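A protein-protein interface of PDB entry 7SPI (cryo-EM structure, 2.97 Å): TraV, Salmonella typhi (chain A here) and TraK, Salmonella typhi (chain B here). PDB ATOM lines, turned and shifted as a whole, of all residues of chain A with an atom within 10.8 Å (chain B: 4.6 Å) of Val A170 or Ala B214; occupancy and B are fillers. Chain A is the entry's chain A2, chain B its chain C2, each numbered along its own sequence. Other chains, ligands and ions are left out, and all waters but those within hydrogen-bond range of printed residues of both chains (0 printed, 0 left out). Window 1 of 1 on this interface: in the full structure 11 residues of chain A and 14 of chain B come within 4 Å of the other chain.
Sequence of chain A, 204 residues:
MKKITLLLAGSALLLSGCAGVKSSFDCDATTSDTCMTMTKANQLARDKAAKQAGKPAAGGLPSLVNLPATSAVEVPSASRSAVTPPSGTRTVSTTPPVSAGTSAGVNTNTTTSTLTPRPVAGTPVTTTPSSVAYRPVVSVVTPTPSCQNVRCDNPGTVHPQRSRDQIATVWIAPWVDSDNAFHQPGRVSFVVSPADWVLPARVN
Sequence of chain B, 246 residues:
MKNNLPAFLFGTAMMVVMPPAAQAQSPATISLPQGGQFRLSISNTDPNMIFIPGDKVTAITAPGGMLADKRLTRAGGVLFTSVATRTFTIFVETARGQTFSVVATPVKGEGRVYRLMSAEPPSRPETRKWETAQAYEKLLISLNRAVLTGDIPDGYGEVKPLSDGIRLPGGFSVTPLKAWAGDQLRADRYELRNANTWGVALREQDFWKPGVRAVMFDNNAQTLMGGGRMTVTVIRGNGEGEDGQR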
ATOM      1  N   ILE A 167     -19.939 -24.300 -17.463  1.00  0.00           N
ATOM      2  CA  ILE A 167     -20.398 -23.900 -16.146  1.00  0.00           C
ATOM      3  C   ILE A 167     -19.288 -23.912 -15.121  1.00  0.00           C
ATOM      4  O   ILE A 167     -18.247 -24.530 -15.332  1.00  0.00           O
ATOM      5  CB  ILE A 167     -21.547 -24.808 -15.652  1.00  0.00           C
ATOM      6  CG1 ILE A 167     -21.052 -26.235 -15.425  1.00  0.00           C
ATOM      7  CG2 ILE A 167     -22.700 -24.792 -16.640  1.00  0.00           C
ATOM      8  CD1 ILE A 167     -22.025 -27.091 -14.648  1.00  0.00           C
ATOM      9  N   ALA A 168     -19.503 -23.222 -14.010  1.00  0.00           N
ATOM     10  CA  ALA A 168     -18.517 -23.228 -12.940  1.00  0.00           C
ATOM     11  C   ALA A 168     -19.233 -23.294 -11.602  1.00  0.00           C
ATOM     12  O   ALA A 168     -20.163 -22.522 -11.347  1.00  0.00           O
ATOM     13  CB  ALA A 168     -17.616 -21.988 -12.995  1.00  0.00           C
ATOM     14  N   THR A 169     -18.796 -24.218 -10.751  1.00  0.00           N
ATOM     15  CA  THR A 169     -19.379 -24.417  -9.428  1.00  0.00           C
ATOM     16  C   THR A 169     -18.327 -24.109  -8.372  1.00  0.00           C
ATOM     17  O   THR A 169     -17.213 -24.641  -8.425  1.00  0.00           O
ATOM     18  CB  THR A 169     -19.894 -25.848  -9.268  1.00  0.00           C
ATOM     19  OG1 THR A 169     -20.423 -26.310 -10.518  1.00  0.00           O
ATOM     20  CG2 THR A 169     -20.983 -25.906  -8.210  1.00  0.00           C
ATOM     21  N   VAL A 170     -18.725 -23.295  -7.386  1.00  0.00           N
ATOM     22  CA  VAL A 170     -17.840 -22.918  -6.286  1.00  0.00           C
ATOM     23  C   VAL A 170     -18.400 -23.408  -4.958  1.00  0.00           C
ATOM     24  O   VAL A 170     -19.523 -23.066  -4.608  1.00  0.00           O
ATOM     25  CB  VAL A 170     -17.777 -21.387  -6.166  1.00  0.00           C
ATOM     26  CG1 VAL A 170     -16.961 -20.978  -4.952  1.00  0.00           C
ATOM     27  CG2 VAL A 170     -17.209 -20.770  -7.431  1.00  0.00           C
ATOM     28  N   TRP A 171     -17.650 -24.221  -4.223  1.00  0.00           N
ATOM     29  CA  TRP A 171     -18.087 -24.651  -2.895  1.00  0.00           C
ATOM     30  C   TRP A 171     -17.970 -23.524  -1.879  1.00  0.00           C
ATOM     31  O   TRP A 171     -16.971 -22.817  -1.858  1.00  0.00           O
ATOM     32  CB  TRP A 171     -17.269 -25.852  -2.447  1.00  0.00           C
ATOM     33  CG  TRP A 171     -17.588 -26.341  -1.083  1.00  0.00           C
ATOM     34  CD1 TRP A 171     -18.662 -27.087  -0.715  1.00  0.00           C
ATOM     35  CD2 TRP A 171     -16.815 -26.133   0.102  1.00  0.00           C
ATOM     36  NE1 TRP A 171     -18.615 -27.349   0.629  1.00  0.00           N
ATOM     37  CE2 TRP A 171     -17.489 -26.776   1.155  1.00  0.00           C
ATOM     38  CE3 TRP A 171     -15.620 -25.460   0.377  1.00  0.00           C
ATOM     39  CZ2 TRP A 171     -17.009 -26.770   2.461  1.00  0.00           C
ATOM     40  CZ3 TRP A 171     -15.147 -25.456   1.670  1.00  0.00           C
ATOM     41  CH2 TRP A 171     -15.839 -26.108   2.698  1.00  0.00           C
ATOM     42  N   ILE A 172     -18.994 -23.369  -1.045  1.00  0.00           N
ATOM     43  CA  ILE A 172     -18.986 -22.334  -0.020  1.00  0.00           C
ATOM     44  C   ILE A 172     -18.814 -22.984   1.340  1.00  0.00           C
ATOM     45  O   ILE A 172     -19.457 -23.991   1.627  1.00  0.00           O
ATOM     46  CB  ILE A 172     -20.323 -21.571  -0.008  1.00  0.00           C
ATOM     47  CG1 ILE A 172     -20.847 -21.373  -1.431  1.00  0.00           C
ATOM     48  CG2 ILE A 172     -20.181 -20.243   0.720  1.00  0.00           C
ATOM     49  CD1 ILE A 172     -22.267 -20.858  -1.484  1.00  0.00           C
ATOM     50  N   ALA A 173     -17.947 -22.426   2.177  1.00  0.00           N
ATOM     51  CA  ALA A 173     -17.767 -22.942   3.531  1.00  0.00           C
ATOM     52  C   ALA A 173     -18.833 -22.451   4.511  1.00  0.00           C
ATOM     53  O   ALA A 173     -19.459 -21.425   4.271  1.00  0.00           O
ATOM     54  CB  ALA A 173     -16.382 -22.583   4.020  1.00  0.00           C
ATOM     55  N   PRO A 174     -19.023 -23.175   5.663  1.00  0.00           N
ATOM     56  CA  PRO A 174     -20.027 -22.663   6.597  1.00  0.00           C
ATOM     57  C   PRO A 174     -19.866 -21.219   7.051  1.00  0.00           C
ATOM     58  O   PRO A 174     -18.744 -20.780   7.293  1.00  0.00           O
ATOM     59  CB  PRO A 174     -19.930 -23.618   7.789  1.00  0.00           C
ATOM     60  CG  PRO A 174     -18.636 -24.327   7.632  1.00  0.00           C
ATOM     61  CD  PRO A 174     -18.469 -24.455   6.164  1.00  0.00           C
ATOM     62  N   TRP A 175     -20.981 -20.502   7.181  1.00  0.00           N
ATOM     63  CA  TRP A 175     -20.915 -19.090   7.551  1.00  0.00           C
ATOM     64  C   TRP A 175     -22.120 -18.545   8.302  1.00  0.00           C
ATOM     65  O   TRP A 175     -23.228 -19.034   8.137  1.00  0.00           O
ATOM     66  CB  TRP A 175     -20.639 -18.225   6.311  1.00  0.00           C
ATOM     67  CG  TRP A 175     -21.669 -18.344   5.224  1.00  0.00           C
ATOM     68  CD1 TRP A 175     -21.815 -19.370   4.336  1.00  0.00           C
ATOM     69  CD2 TRP A 175     -22.682 -17.387   4.896  1.00  0.00           C
ATOM     70  NE1 TRP A 175     -22.861 -19.119   3.485  1.00  0.00           N
ATOM     71  CE2 TRP A 175     -23.410 -17.907   3.807  1.00  0.00           C
ATOM     72  CE3 TRP A 175     -23.048 -16.145   5.420  1.00  0.00           C
ATOM     73  CZ2 TRP A 175     -24.481 -17.227   3.234  1.00  0.00           C
ATOM     74  CZ3 TRP A 175     -24.109 -15.472   4.847  1.00  0.00           C
ATOM     75  CH2 TRP A 175     -24.815 -16.015   3.768  1.00  0.00           C
ATOM     76  N   GLN A 184     -24.643 -24.014   6.683  1.00  0.00           N
ATOM     77  CA  GLN A 184     -23.767 -25.158   6.447  1.00  0.00           C
ATOM     78  C   GLN A 184     -23.214 -25.144   5.024  1.00  0.00           C
ATOM     79  O   GLN A 184     -23.770 -24.479   4.148  1.00  0.00           O
ATOM     80  CB  GLN A 184     -24.542 -26.455   6.706  1.00  0.00           C
ATOM     81  CG  GLN A 184     -25.018 -26.618   8.137  1.00  0.00           C
ATOM     82  CD  GLN A 184     -25.437 -28.042   8.443  1.00  0.00           C
ATOM     83  OE1 GLN A 184     -25.119 -28.967   7.698  1.00  0.00           O
ATOM     84  NE2 GLN A 184     -26.147 -28.225   9.550  1.00  0.00           N
ATOM     85  N   PRO A 185     -22.092 -25.890   4.792  1.00  0.00           N
ATOM     86  CA  PRO A 185     -21.515 -25.781   3.446  1.00  0.00           C
ATOM     87  C   PRO A 185     -22.410 -26.129   2.280  1.00  0.00           C
ATOM     88  O   PRO A 185     -23.088 -27.157   2.298  1.00  0.00           O
ATOM     89  CB  PRO A 185     -20.315 -26.735   3.480  1.00  0.00           C
ATOM     90  CG  PRO A 185     -20.475 -27.563   4.689  1.00  0.00           C
ATOM     91  CD  PRO A 185     -21.222 -26.723   5.658  1.00  0.00           C
ATOM     92  N   GLY A 186     -22.402 -25.278   1.270  1.00  0.00           N
ATOM     93  CA  GLY A 186     -23.174 -25.504   0.066  1.00  0.00           C
ATOM     94  C   GLY A 186     -22.398 -25.155  -1.184  1.00  0.00           C
ATOM     95  O   GLY A 186     -21.167 -25.077  -1.154  1.00  0.00           O
ATOM     96  N   ARG A 187     -23.102 -24.939  -2.296  1.00  0.00           N
ATOM     97  CA  ARG A 187     -22.447 -24.596  -3.547  1.00  0.00           C
ATOM     98  C   ARG A 187     -23.398 -23.786  -4.415  1.00  0.00           C
ATOM     99  O   ARG A 187     -24.619 -23.875  -4.277  1.00  0.00           O
ATOM    100  CB  ARG A 187     -21.981 -25.848  -4.299  1.00  0.00           C
ATOM    101  CG  ARG A 187     -23.092 -26.831  -4.612  1.00  0.00           C
ATOM    102  CD  ARG A 187     -22.549 -28.070  -5.301  1.00  0.00           C
ATOM    103  NE  ARG A 187     -21.787 -28.911  -4.385  1.00  0.00           N
ATOM    104  CZ  ARG A 187     -20.482 -29.127  -4.479  1.00  0.00           C
ATOM    105  NH1 ARG A 187     -19.756 -28.572  -5.436  1.00  0.00           N
ATOM    106  NH2 ARG A 187     -19.891 -29.919  -3.591  1.00  0.00           N
ATOM    107  N   VAL A 188     -22.827 -22.969  -5.305  1.00  0.00           N
ATOM    108  CA  VAL A 188     -23.626 -22.155  -6.232  1.00  0.00           C
ATOM    109  C   VAL A 188     -22.987 -22.228  -7.623  1.00  0.00           C
ATOM    110  O   VAL A 188     -21.768 -22.122  -7.750  1.00  0.00           O
ATOM    111  CB  VAL A 188     -23.738 -20.691  -5.760  1.00  0.00           C
ATOM    112  CG1 VAL A 188     -24.461 -19.832  -6.786  1.00  0.00           C
ATOM    113  CG2 VAL A 188     -24.390 -20.595  -4.390  1.00  0.00           C
ATOM    114  N   SER A 189     -23.791 -22.447  -8.660  1.00  0.00           N
ATOM    115  CA  SER A 189     -23.246 -22.590 -10.009  1.00  0.00           C
ATOM    116  C   SER A 189     -23.551 -21.392 -10.894  1.00  0.00           C
ATOM    117  O   SER A 189     -24.654 -20.846 -10.834  1.00  0.00           O
ATOM    118  CB  SER A 189     -23.798 -23.853 -10.673  1.00  0.00           C
ATOM    119  OG  SER A 189     -25.200 -23.769 -10.853  1.00  0.00           O
ATOM    120  N   PHE A 190     -22.589 -20.978 -11.716  1.00  0.00           N
ATOM    121  CA  PHE A 190     -22.844 -19.892 -12.651  1.00  0.00           C
ATOM    122  C   PHE A 190     -22.281 -20.263 -14.006  1.00  0.00           C
ATOM    123  O   PHE A 190     -21.434 -21.140 -14.106  1.00  0.00           O
ATOM    124  CB  PHE A 190     -22.252 -18.571 -12.156  1.00  0.00           C
ATOM    125  CG  PHE A 190     -20.761 -18.590 -11.969  1.00  0.00           C
ATOM    126  CD1 PHE A 190     -20.202 -19.073 -10.800  1.00  0.00           C
ATOM    127  CD2 PHE A 190     -19.918 -18.098 -12.952  1.00  0.00           C
ATOM    128  CE1 PHE A 190     -18.835 -19.089 -10.625  1.00  0.00           C
ATOM    129  CE2 PHE A 190     -18.550 -18.110 -12.784  1.00  0.00           C
ATOM    130  CZ  PHE A 190     -18.008 -18.605 -11.616  1.00  0.00           C
ATOM    131  N   VAL A 191     -22.770 -19.612 -15.056  1.00  0.00           N
ATOM    132  CA  VAL A 191     -22.294 -19.907 -16.405  1.00  0.00           C
ATOM    133  C   VAL A 191     -21.232 -18.905 -16.813  1.00  0.00           C
ATOM    134  O   VAL A 191     -21.482 -17.703 -16.828  1.00  0.00           O
ATOM    135  CB  VAL A 191     -23.450 -19.918 -17.429  1.00  0.00           C
ATOM    136  CG1 VAL A 191     -22.939 -20.186 -18.834  1.00  0.00           C
ATOM    137  CG2 VAL A 191     -24.492 -20.947 -17.038  1.00  0.00           C
ATOM    138  N   VAL A 192     -20.044 -19.396 -17.143  1.00  0.00           N
ATOM    139  CA  VAL A 192     -18.945 -18.518 -17.514  1.00  0.00           C
ATOM    140  C   VAL A 192     -19.007 -18.160 -18.997  1.00  0.00           C
ATOM    141  O   VAL A 192     -18.952 -16.982 -19.348  1.00  0.00           O
ATOM    142  CB  VAL A 192     -17.592 -19.144 -17.116  1.00  0.00           C
ATOM    143  CG1 VAL A 192     -16.422 -18.309 -17.598  1.00  0.00           C
ATOM    144  CG2 VAL A 192     -17.519 -19.412 -15.621  1.00  0.00           C
ATOM    145  N   LEU B 140     -19.214 -13.573  -3.615  1.00  0.00           N
ATOM    146  CA  LEU B 140     -18.350 -14.721  -3.860  1.00  0.00           C
ATOM    147  C   LEU B 140     -18.355 -15.065  -5.340  1.00  0.00           C
ATOM    148  O   LEU B 140     -17.298 -15.252  -5.937  1.00  0.00           O
ATOM    149  CB  LEU B 140     -18.809 -15.934  -3.053  1.00  0.00           C
ATOM    150  CG  LEU B 140     -18.774 -15.845  -1.529  1.00  0.00           C
ATOM    151  CD1 LEU B 140     -19.188 -17.187  -0.947  1.00  0.00           C
ATOM    152  CD2 LEU B 140     -17.389 -15.455  -1.035  1.00  0.00           C
ATOM    153  N   ASN B 144     -15.083 -14.791  -7.910  1.00  0.00           N
ATOM    154  CA  ASN B 144     -14.701 -16.001  -8.606  1.00  0.00           C
ATOM    155  C   ASN B 144     -14.821 -15.862 -10.118  1.00  0.00           C
ATOM    156  O   ASN B 144     -14.027 -16.409 -10.853  1.00  0.00           O
ATOM    157  CB  ASN B 144     -15.488 -17.179  -8.056  1.00  0.00           C
ATOM    158  CG  ASN B 144     -14.815 -17.844  -6.885  1.00  0.00           C
ATOM    159  OD1 ASN B 144     -13.616 -18.102  -6.905  1.00  0.00           O
ATOM    160  ND2 ASN B 144     -15.590 -18.150  -5.864  1.00  0.00           N
ATOM    161  N   VAL B 212     -10.674 -20.279   4.948  1.00  0.00           N
ATOM    162  CA  VAL B 212     -10.972 -20.493   3.551  1.00  0.00           C
ATOM    163  C   VAL B 212     -12.432 -20.346   3.446  1.00  0.00           C
ATOM    164  O   VAL B 212     -13.170 -21.125   4.002  1.00  0.00           O
ATOM    165  CB  VAL B 212     -10.574 -21.876   3.107  1.00  0.00           C
ATOM    166  CG1 VAL B 212     -11.046 -22.134   1.690  1.00  0.00           C
ATOM    167  CG2 VAL B 212      -9.077 -22.050   3.205  1.00  0.00           C
ATOM    168  N   ARG B 213     -12.870 -19.344   2.741  1.00  0.00           N
ATOM    169  CA  ARG B 213     -14.290 -19.033   2.665  1.00  0.00           C
ATOM    170  C   ARG B 213     -14.997 -19.720   1.506  1.00  0.00           C
ATOM    171  O   ARG B 213     -16.178 -20.054   1.628  1.00  0.00           O
ATOM    172  CB  ARG B 213     -14.457 -17.510   2.557  1.00  0.00           C
ATOM    173  CG  ARG B 213     -15.808 -16.992   2.990  1.00  0.00           C
ATOM    174  CD  ARG B 213     -15.684 -15.609   3.604  1.00  0.00           C
ATOM    175  NE  ARG B 213     -14.700 -15.579   4.679  1.00  0.00           N
ATOM    176  CZ  ARG B 213     -14.916 -15.052   5.879  1.00  0.00           C
ATOM    177  NH1 ARG B 213     -16.075 -14.497   6.190  1.00  0.00           N
ATOM    178  NH2 ARG B 213     -13.944 -15.084   6.783  1.00  0.00           N
ATOM    179  N   ALA B 214     -14.308 -19.942   0.388  1.00  0.00           N
ATOM    180  CA  ALA B 214     -14.910 -20.587  -0.771  1.00  0.00           C
ATOM    181  C   ALA B 214     -13.815 -21.192  -1.636  1.00  0.00           C
ATOM    182  O   ALA B 214     -12.693 -20.682  -1.687  1.00  0.00           O
ATOM    183  CB  ALA B 214     -15.751 -19.605  -1.591  1.00  0.00           C
ATOM    184  N   VAL B 215     -14.153 -22.288  -2.313  1.00  0.00           N
ATOM    185  CA  VAL B 215     -13.235 -22.996  -3.197  1.00  0.00           C
ATOM    186  C   VAL B 215     -13.961 -23.320  -4.495  1.00  0.00           C
ATOM    187  O   VAL B 215     -15.098 -23.803  -4.474  1.00  0.00           O
ATOM    188  CB  VAL B 215     -12.695 -24.287  -2.543  1.00  0.00           C
ATOM    189  CG1 VAL B 215     -11.809 -25.049  -3.513  1.00  0.00           C
ATOM    190  CG2 VAL B 215     -11.934 -23.967  -1.268  1.00  0.00           C
ATOM    191  N   MET B 216     -13.304 -23.056  -5.625  1.00  0.00           N
ATOM    192  CA  MET B 216     -13.856 -23.394  -6.930  1.00  0.00           C
ATOM    193  C   MET B 216     -12.776 -24.045  -7.779  1.00  0.00           C
ATOM    194  O   MET B 216     -11.625 -23.602  -7.780  1.00  0.00           O
ATOM    195  CB  MET B 216     -14.407 -22.158  -7.661  1.00  0.00           C
ATOM    196  CG  MET B 216     -14.277 -22.241  -9.183  1.00  0.00           C
ATOM    197  SD  MET B 216     -14.897 -20.822 -10.105  1.00  0.00           S
ATOM    198  CE  MET B 216     -13.530 -19.681  -9.936  1.00  0.00           C
ATOM    199  N   THR B 233      -9.142 -21.780  -7.287  1.00  0.00           N
ATOM    200  CA  THR B 233      -9.209 -20.431  -6.757  1.00  0.00           C
ATOM    201  C   THR B 233      -9.855 -20.459  -5.385  1.00  0.00           C
ATOM    202  O   THR B 233     -10.966 -20.965  -5.230  1.00  0.00           O
ATOM    203  CB  THR B 233     -10.040 -19.516  -7.661  1.00  0.00           C
ATOM    204  OG1 THR B 233      -9.508 -19.542  -8.991  1.00  0.00           O
ATOM    205  CG2 THR B 233     -10.010 -18.093  -7.134  1.00  0.00           C
ATOM    206  N   VAL B 234      -9.165 -19.916  -4.386  1.00  0.00           N
ATOM    207  CA  VAL B 234      -9.727 -19.870  -3.043  1.00  0.00           C
ATOM    208  C   VAL B 234      -9.937 -18.457  -2.523  1.00  0.00           C
ATOM    209  O   VAL B 234      -9.080 -17.589  -2.679  1.00  0.00           O
ATOM    210  CB  VAL B 234      -8.950 -20.755  -2.034  1.00  0.00           C
ATOM    211  CG1 VAL B 234      -8.442 -22.012  -2.718  1.00  0.00           C
ATOM    212  CG2 VAL B 234      -7.814 -20.004  -1.364  1.00  0.00           C
ATOM    213  N   ILE B 235     -11.113 -18.202  -1.967  1.00  0.00           N
ATOM    214  CA  ILE B 235     -11.380 -16.901  -1.380  1.00  0.00           C
ATOM    215  C   ILE B 235     -11.251 -17.121   0.104  1.00  0.00           C
ATOM    216  O   ILE B 235     -11.644 -18.167   0.599  1.00  0.00           O
ATOM    217  CB  ILE B 235     -12.786 -16.390  -1.718  1.00  0.00           C
ATOM    218  CG1 ILE B 235     -13.023 -16.444  -3.225  1.00  0.00           C
ATOM    219  CG2 ILE B 235     -12.981 -14.970  -1.213  1.00  0.00           C
ATOM    220  CD1 ILE B 235     -14.311 -15.782  -3.654  1.00  0.00           C
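Among the printed residues, merely in contact across the chains: Thr A169 with Met B216 (3.8 Å), Val A170 with Asn B144 (3.3 Å), Val A170 with Ala B214 (3.8 Å), Val A170 with Val B215 (3.4 Å), Val A170 with Met B216 (3.1 Å), Trp A171 with Ala B214 (3.2 Å), Ile A172 with Leu B140 (3.6 Å), Ile A172 with Arg B213 (3.95 Å) and Ala A173 with Val B212 (3.5 Å).
Ala B214 touches just these residues of chain A: Val A170 (3.8 Å) and Trp A171 (3.2 Å). Printed residues of chain A within 4 Å of Asn B144: Val A170 (3.3 Å). Of chain A, only Ala A173 comes within 4 Å of Val B212. Met B216 touches two residues of chain A. Val B234 touches none of the printed residues of chain A. No residue of chain A comes within 4 Å of Ile B235. Of the printed residues of chain B, Thr A169 touches Met B216. Of the printed residues of chain A, Arg B213 touches Ile A172 and Ala A173. Printed residues of chain B within 4 Å of Trp A171: Ala B214 and Val B215. Ala A168 touches none of the printed residues of chain B. The nearest printed residue of chain B that does not touch Val A170 is Leu B140 (5.7 Å). The nearest residue of chain A that does not touch Ala B214 is Ile A172 (4.5 Å). The nearest printed residue of chain B that does not touch Ile A172 is Ala B214 (4.5 Å).
The backbone NH (N) of Trp A171 lies within hydrogen-bond range of the backbone carbonyl oxygen (O) of Val B215. The backbone carbonyl oxygen (O) of Arg B213 is in hydrogen-bond range of the backbone NH (N) of Ala A173 (3.0 Å).
The backbone NH of Val A170 is in hydrogen-bond range of the backbone carbonyl oxygen of Val A188 (3.3 Å). O of Gly A186 sits at hydrogen-bond distance from N of Ile A172, 2.8 Å away. The backbone carbonyl oxygen (O) of Leu B140 is in hydrogen-bond range of the side-chain amide nitrogen (ND2) of Asn B144 (3.4 Å). The backbone NH (N) of Arg B213 sits at hydrogen-bond distance from the backbone carbonyl oxygen (O) of Ile B235, at 2.7 Å. The backbone carbonyl oxygen (O) of Ala B214 is in hydrogen-bond range of the backbone NH (N) of Ile B235 (3.0 Å). O of Met B216 is in hydrogen-bond range of N of Thr B233, at 3.1 Å.
Printed residues of chain B that touch a printed residue of chain A: Leu B140, Asn B144, Val B212, Arg B213, Ala B214, Val B215 and Met B216. Hydrophobic or aromatic side chains of chain B within 4 Å of the printed part of chain A: Leu B140, Ala B214 and Met B216. Hydrophobic or aromatic side chains of chain A within 4 Å of the printed part of chain B: Val A170, Trp A171, Ile A172 and Ala A173. Among the printed residues, 11 pairs touch across the chains.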
